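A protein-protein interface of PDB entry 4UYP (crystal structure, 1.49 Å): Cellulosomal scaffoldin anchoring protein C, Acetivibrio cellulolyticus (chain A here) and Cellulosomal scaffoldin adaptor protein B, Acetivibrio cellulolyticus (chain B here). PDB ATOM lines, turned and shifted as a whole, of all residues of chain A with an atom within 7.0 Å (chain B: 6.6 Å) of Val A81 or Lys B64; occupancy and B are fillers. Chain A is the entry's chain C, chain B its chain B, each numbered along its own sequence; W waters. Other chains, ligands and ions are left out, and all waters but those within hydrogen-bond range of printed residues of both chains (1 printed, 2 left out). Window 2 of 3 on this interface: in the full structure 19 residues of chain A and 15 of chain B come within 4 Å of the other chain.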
ATOM      1  N   TYR A  32      16.134 -13.333 -25.719  1.00  0.00           N
ATOM      2  CA  TYR A  32      16.843 -14.370 -26.455  1.00  0.00           C
ATOM      3  C   TYR A  32      17.039 -14.032 -27.940  1.00  0.00           C
ATOM      4  O   TYR A  32      17.988 -14.520 -28.565  1.00  0.00           O
ATOM      5  CB  TYR A  32      15.946 -15.640 -26.278  1.00  0.00           C
ATOM      6  CG  TYR A  32      16.493 -16.914 -26.857  1.00  0.00           C
ATOM      7  CD1 TYR A  32      17.708 -17.450 -26.345  1.00  0.00           C
ATOM      8  CD2 TYR A  32      15.882 -17.589 -27.884  1.00  0.00           C
ATOM      9  CE1 TYR A  32      18.182 -18.668 -26.831  1.00  0.00           C
ATOM     10  CE2 TYR A  32      16.338 -18.839 -28.377  1.00  0.00           C
ATOM     11  CZ  TYR A  32      17.501 -19.343 -27.849  1.00  0.00           C
ATOM     12  OH  TYR A  32      18.002 -20.547 -28.288  1.00  0.00           O
ATOM     13  N   GLU A  78      20.610 -12.875 -31.788  1.00  0.00           N
ATOM     14  CA  GLU A  78      20.205 -14.267 -31.495  1.00  0.00           C
ATOM     15  C   GLU A  78      21.147 -14.747 -30.399  1.00  0.00           C
ATOM     16  O   GLU A  78      22.361 -14.953 -30.713  1.00  0.00           O
ATOM     17  CB  GLU A  78      20.307 -15.103 -32.722  1.00  0.00           C
ATOM     18  CG  GLU A  78      19.411 -14.662 -33.930  1.00  0.00           C
ATOM     19  CD  GLU A  78      20.012 -15.125 -35.298  1.00  0.00           C
ATOM     20  OE1 GLU A  78      21.189 -14.772 -35.618  1.00  0.00           O
ATOM     21  OE2 GLU A  78      19.178 -15.844 -35.934  1.00  0.00           O
ATOM     22  N   ALA A  79      20.690 -14.891 -29.174  1.00  0.00           N
ATOM     23  CA  ALA A  79      21.552 -15.477 -28.161  1.00  0.00           C
ATOM     24  C   ALA A  79      21.933 -16.886 -28.538  1.00  0.00           C
ATOM     25  O   ALA A  79      21.214 -17.552 -29.261  1.00  0.00           O
ATOM     26  CB  ALA A  79      20.802 -15.510 -26.873  1.00  0.00           C
ATOM     27  N   PRO A  80      23.099 -17.304 -28.091  1.00  0.00           N
ATOM     28  CA  PRO A  80      23.427 -18.724 -28.325  1.00  0.00           C
ATOM     29  C   PRO A  80      22.452 -19.651 -27.580  1.00  0.00           C
ATOM     30  O   PRO A  80      21.775 -19.220 -26.626  1.00  0.00           O
ATOM     31  CB  PRO A  80      24.883 -18.796 -27.739  1.00  0.00           C
ATOM     32  CG  PRO A  80      24.877 -17.753 -26.633  1.00  0.00           C
ATOM     33  CD  PRO A  80      24.109 -16.592 -27.304  1.00  0.00           C
ATOM     34  N   VAL A  81      22.519 -20.915 -28.006  1.00  0.00           N
ATOM     35  CA  VAL A  81      21.481 -21.867 -27.532  1.00  0.00           C
ATOM     36  C   VAL A  81      21.546 -22.154 -26.068  1.00  0.00           C
ATOM     37  O   VAL A  81      20.527 -22.524 -25.451  1.00  0.00           O
ATOM     38  CB  VAL A  81      21.474 -23.213 -28.245  1.00  0.00           C
ATOM     39  CG1 VAL A  81      20.130 -23.924 -27.999  1.00  0.00           C
ATOM     40  CG2 VAL A  81      21.614 -23.023 -29.696  1.00  0.00           C
ATOM     41  N   ASP A  82      22.712 -21.962 -25.446  1.00  0.00           N
ATOM     42  CA  ASP A  82      22.887 -22.047 -24.007  1.00  0.00           C
ATOM     43  C   ASP A  82      22.666 -20.825 -23.223  1.00  0.00           C
ATOM     44  O   ASP A  82      22.943 -20.752 -22.019  1.00  0.00           O
ATOM     45  CB  ASP A  82      24.264 -22.684 -23.676  1.00  0.00           C
ATOM     46  CG  ASP A  82      25.465 -21.860 -24.213  1.00  0.00           C
ATOM     47  OD1 ASP A  82      25.199 -20.789 -24.906  1.00  0.00           O
ATOM     48  OD2 ASP A  82      26.660 -22.189 -23.956  1.00  0.00           O
ATOM     49  N   ARG A  83      22.163 -19.733 -23.886  1.00  0.00           N
ATOM     50  CA  ARG A  83      22.053 -18.487 -23.256  1.00  0.00           C
ATOM     51  C   ARG A  83      23.377 -18.006 -22.586  1.00  0.00           C
ATOM     52  O   ARG A  83      23.307 -17.121 -21.672  1.00  0.00           O
ATOM     53  CB  ARG A  83      20.910 -18.472 -22.255  1.00  0.00           C
ATOM     54  CG  ARG A  83      19.581 -18.797 -22.725  1.00  0.00           C
ATOM     55  CD  ARG A  83      18.819 -18.066 -21.567  1.00  0.00           C
ATOM     56  NE  ARG A  83      17.543 -17.981 -21.989  1.00  0.00           N
ATOM     57  CZ  ARG A  83      16.624 -17.087 -22.325  1.00  0.00           C
ATOM     58  NH1 ARG A  83      15.842 -17.675 -23.225  1.00  0.00           N
ATOM     59  NH2 ARG A  83      16.236 -15.887 -21.826  1.00  0.00           N
ATOM     60  N   ALA A  84      24.536 -18.390 -23.118  1.00  0.00           N
ATOM     61  CA  ALA A  84      25.865 -17.939 -22.573  1.00  0.00           C
ATOM     62  C   ALA A  84      26.017 -16.428 -22.722  1.00  0.00           C
ATOM     63  O   ALA A  84      26.764 -15.770 -21.965  1.00  0.00           O
ATOM     64  CB  ALA A  84      27.063 -18.670 -23.195  1.00  0.00           C
ATOM     65  N   ARG A  85      25.286 -15.854 -23.680  1.00  0.00           N
ATOM     66  CA  ARG A  85      25.223 -14.382 -23.805  1.00  0.00           C
ATOM     67  C   ARG A  85      23.721 -14.188 -23.880  1.00  0.00           C
ATOM     68  O   ARG A  85      23.013 -15.042 -24.442  1.00  0.00           O
ATOM     69  CB  ARG A  85      25.855 -13.842 -25.134  1.00  0.00           C
ATOM     70  CG  ARG A  85      27.370 -13.681 -25.139  1.00  0.00           C
ATOM     71  CD  ARG A  85      28.127 -14.785 -25.704  1.00  0.00           C
ATOM     72  NE  ARG A  85      27.709 -15.236 -27.012  1.00  0.00           N
ATOM     73  CZ  ARG A  85      28.124 -16.357 -27.592  1.00  0.00           C
ATOM     74  NH1 ARG A  85      29.004 -17.223 -26.909  1.00  0.00           N
ATOM     75  NH2 ARG A  85      27.762 -16.678 -28.813  1.00  0.00           N
ATOM     76  N   SER A 124      12.150 -16.220 -25.601  1.00  0.00           N
ATOM     77  CA  SER A 124      12.619 -17.572 -25.949  1.00  0.00           C
ATOM     78  C   SER A 124      12.140 -17.814 -27.345  1.00  0.00           C
ATOM     79  O   SER A 124      11.494 -16.921 -27.956  1.00  0.00           O
ATOM     80  CB  SER A 124      11.880 -18.564 -24.977  1.00  0.00           C
ATOM     81  OG  SER A 124      10.506 -18.652 -25.402  1.00  0.00           O
ATOM     82  N   GLY A 125      12.424 -18.977 -27.895  1.00  0.00           N
ATOM     83  CA  GLY A 125      12.040 -19.212 -29.252  1.00  0.00           C
ATOM     84  C   GLY A 125      10.533 -19.113 -29.448  1.00  0.00           C
ATOM     85  O   GLY A 125      10.097 -18.919 -30.647  1.00  0.00           O
ATOM     86  N   VAL B  55      15.573 -18.591 -35.116  1.00  0.00           N
ATOM     87  CA  VAL B  55      16.239 -19.183 -33.981  1.00  0.00           C
ATOM     88  C   VAL B  55      15.674 -20.577 -33.677  1.00  0.00           C
ATOM     89  O   VAL B  55      16.463 -21.443 -33.274  1.00  0.00           O
ATOM     90  CB  VAL B  55      16.288 -18.250 -32.780  1.00  0.00           C
ATOM     91  CG1 VAL B  55      14.983 -18.224 -31.953  1.00  0.00           C
ATOM     92  CG2 VAL B  55      17.568 -18.458 -32.001  1.00  0.00           C
ATOM     93  N   ARG B  58      17.550 -22.827 -36.066  1.00  0.00           N
ATOM     94  CA  ARG B  58      18.881 -23.073 -35.551  1.00  0.00           C
ATOM     95  C   ARG B  58      18.859 -24.032 -34.372  1.00  0.00           C
ATOM     96  O   ARG B  58      19.684 -24.965 -34.322  1.00  0.00           O
ATOM     97  CB  ARG B  58      19.445 -21.739 -35.092  1.00  0.00           C
ATOM     98  CG  ARG B  58      20.866 -21.975 -34.600  1.00  0.00           C
ATOM     99  CD  ARG B  58      21.294 -20.791 -33.801  1.00  0.00           C
ATOM    100  NE  ARG B  58      20.570 -20.743 -32.506  1.00  0.00           N
ATOM    101  CZ  ARG B  58      20.742 -19.813 -31.594  1.00  0.00           C
ATOM    102  NH1 ARG B  58      21.557 -18.754 -31.808  1.00  0.00           N
ATOM    103  NH2 ARG B  58      20.050 -19.865 -30.429  1.00  0.00           N
ATOM    104  N   ASP B  59      17.905 -23.804 -33.470  1.00  0.00           N
ATOM    105  CA  ASP B  59      17.836 -24.653 -32.235  1.00  0.00           C
ATOM    106  C   ASP B  59      17.441 -26.055 -32.605  1.00  0.00           C
ATOM    107  O   ASP B  59      17.939 -26.976 -31.901  1.00  0.00           O
ATOM    108  CB  ASP B  59      16.896 -24.014 -31.228  1.00  0.00           C
ATOM    109  CG  ASP B  59      17.441 -22.696 -30.659  1.00  0.00           C
ATOM    110  OD1 ASP B  59      18.631 -22.349 -30.916  1.00  0.00           O
ATOM    111  OD2 ASP B  59      16.686 -22.049 -29.930  1.00  0.00           O
ATOM    112  N   TYR B  60      16.637 -26.279 -33.598  1.00  0.00           N
ATOM    113  CA  TYR B  60      16.396 -27.674 -34.036  1.00  0.00           C
ATOM    114  C   TYR B  60      17.703 -28.294 -34.564  1.00  0.00           C
ATOM    115  O   TYR B  60      18.056 -29.455 -34.244  1.00  0.00           O
ATOM    116  CB  TYR B  60      15.328 -27.672 -35.154  1.00  0.00           C
ATOM    117  CG  TYR B  60      15.086 -28.982 -35.821  1.00  0.00           C
ATOM    118  CD1 TYR B  60      14.138 -29.845 -35.270  1.00  0.00           C
ATOM    119  CD2 TYR B  60      15.760 -29.363 -36.957  1.00  0.00           C
ATOM    120  CE1 TYR B  60      13.906 -31.097 -35.823  1.00  0.00           C
ATOM    121  CE2 TYR B  60      15.453 -30.596 -37.561  1.00  0.00           C
ATOM    122  CZ  TYR B  60      14.527 -31.439 -36.972  1.00  0.00           C
ATOM    123  OH  TYR B  60      14.355 -32.686 -37.655  1.00  0.00           O
ATOM    124  N   VAL B  61      18.417 -27.568 -35.434  1.00  0.00           N
ATOM    125  CA  VAL B  61      19.661 -28.089 -35.990  1.00  0.00           C
ATOM    126  C   VAL B  61      20.601 -28.501 -34.863  1.00  0.00           C
ATOM    127  O   VAL B  61      21.292 -29.529 -34.952  1.00  0.00           O
ATOM    128  CB  VAL B  61      20.287 -27.066 -36.951  1.00  0.00           C
ATOM    129  CG1 VAL B  61      21.679 -27.550 -37.346  1.00  0.00           C
ATOM    130  CG2 VAL B  61      19.401 -26.957 -38.204  1.00  0.00           C
ATOM    131  N   LEU B  62      20.686 -27.661 -33.824  1.00  0.00           N
ATOM    132  CA  LEU B  62      21.646 -27.881 -32.713  1.00  0.00           C
ATOM    133  C   LEU B  62      21.138 -28.941 -31.734  1.00  0.00           C
ATOM    134  O   LEU B  62      21.898 -29.262 -30.794  1.00  0.00           O
ATOM    135  CB  LEU B  62      21.954 -26.543 -32.023  1.00  0.00           C
ATOM    136  CG  LEU B  62      22.603 -25.538 -32.952  1.00  0.00           C
ATOM    137  CD1 LEU B  62      22.877 -24.218 -32.246  1.00  0.00           C
ATOM    138  CD2 LEU B  62      23.953 -26.013 -33.579  1.00  0.00           C
ATOM    139  N   GLY B  63      19.923 -29.387 -31.871  1.00  0.00           N
ATOM    140  CA  GLY B  63      19.481 -30.463 -31.020  1.00  0.00           C
ATOM    141  C   GLY B  63      18.787 -30.024 -29.762  1.00  0.00           C
ATOM    142  O   GLY B  63      18.587 -30.841 -28.874  1.00  0.00           O
ATOM    143  N   LYS B  64      18.347 -28.775 -29.642  1.00  0.00           N
ATOM    144  CA  LYS B  64      17.598 -28.332 -28.468  1.00  0.00           C
ATOM    145  C   LYS B  64      16.182 -28.796 -28.541  1.00  0.00           C
ATOM    146  O   LYS B  64      15.565 -29.151 -27.481  1.00  0.00           O
ATOM    147  CB  LYS B  64      17.594 -26.763 -28.435  1.00  0.00           C
ATOM    148  CG  LYS B  64      16.767 -26.219 -27.266  1.00  0.00           C
ATOM    149  CD  LYS B  64      16.346 -24.780 -27.495  1.00  0.00           C
ATOM    150  CE  LYS B  64      15.297 -24.332 -26.478  1.00  0.00           C
ATOM    151  NZ  LYS B  64      15.964 -23.974 -25.153  1.00  0.00           N
ATOM    152  N   ILE B  65      15.586 -28.803 -29.738  1.00  0.00           N
ATOM    153  CA  ILE B  65      14.214 -29.243 -29.918  1.00  0.00           C
ATOM    154  C   ILE B  65      14.226 -30.282 -31.028  1.00  0.00           C
ATOM    155  O   ILE B  65      15.137 -30.340 -31.890  1.00  0.00           O
ATOM    156  CB  ILE B  65      13.238 -28.069 -30.296  1.00  0.00           C
ATOM    157  CG1 ILE B  65      13.642 -27.358 -31.615  1.00  0.00           C
ATOM    158  CG2 ILE B  65      13.076 -27.154 -29.057  1.00  0.00           C
ATOM    159  CD1 ILE B  65      12.616 -26.273 -31.974  1.00  0.00           C
ATOM    160  N   PHE B  66      13.201 -31.147 -31.015  1.00  0.00           N
ATOM    161  CA  PHE B  66      13.142 -32.278 -31.955  1.00  0.00           C
ATOM    162  C   PHE B  66      12.008 -32.231 -32.917  1.00  0.00           C
ATOM    163  O   PHE B  66      11.826 -33.093 -33.777  1.00  0.00           O
ATOM    164  CB  PHE B  66      13.176 -33.618 -31.159  1.00  0.00           C
ATOM    165  CG  PHE B  66      14.387 -33.704 -30.302  1.00  0.00           C
ATOM    166  CD1 PHE B  66      15.630 -33.915 -30.863  1.00  0.00           C
ATOM    167  CD2 PHE B  66      14.270 -33.444 -28.942  1.00  0.00           C
ATOM    168  CE1 PHE B  66      16.777 -33.924 -30.050  1.00  0.00           C
ATOM    169  CE2 PHE B  66      15.370 -33.426 -28.128  1.00  0.00           C
ATOM    170  CZ  PHE B  66      16.627 -33.682 -28.690  1.00  0.00           C
HETATM  171  O   HOH W   1      18.057 -22.051 -25.900  1.00  0.00           O
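The side-chain hydroxyl of Tyr A32 is in hydrogen-bond range of the guanidinium group of Arg B58, at 3.0 Å.
NH1 of Arg B58 is in hydrogen-bond range of O of Ala A79.
The side-chain hydroxyl (OH) of Tyr A32 sits at hydrogen-bond distance from the side-chain carboxylate (OD2) of Asp B59.
The guanidinium group (NH2) of Arg B58 lies within salt-bridge range of the side-chain carboxylate (OD1) of Asp B59 (2.9 Å).
The backbone carbonyl oxygen of Tyr A32 sits at hydrogen-bond distance from the backbone NH of Ala A79, at 2.8 Å.
The backbone carbonyl oxygen of Asp B59 is in hydrogen-bond range of the backbone NH of Lys B64 (2.9 Å).
Among the printed residues, pairs that only touch across the chains: Tyr A32 with Val B55 (3.8 Å), Glu A78 with Arg B58 (3.97 Å), Pro A80 with Arg B58 (3.7 Å), Val A81 with Arg B58 (3.6 Å), Val A81 with Asp B59 (3.3 Å), Val A81 with Leu B62 (3.1 Å) and Val A81 with Lys B64 (3.8 Å).
Printed residues of chain A within 4 Å of Lys B64: Val A81 (3.8 Å).
No residue of chain A comes within 4 Å of Gly B63.
Of the printed residues of chain A, Val B55 touches Tyr A32.
Of the printed residues of chain A, Asp B59 touches Tyr A32 and Val A81.
Of the printed residues of chain A, Leu B62 touches Val A81.
Printed residues of chain A within 4 Å of Arg B58: Tyr A32, Glu A78, Ala A79, Pro A80 and Val A81.
Asp A82 touches none of the printed residues of chain B.
The nearest printed residue of chain A that does not touch Lys B64 is Tyr A32 (4.6 Å).
Printed residues of chain A that touch a printed residue of chain B: Tyr A32, Glu A78, Ala A79, Pro A80 and Val A81.
Hydrophobic or aromatic side chains of chain A that line the printed part of chain B: Tyr A32 and Val A81.
Among the printed residues, 10 pairs touch across the chains.
Water W1 lies within hydrogen-bond range of O of Val A81, OH of Tyr A32 and NZ of Lys B64.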
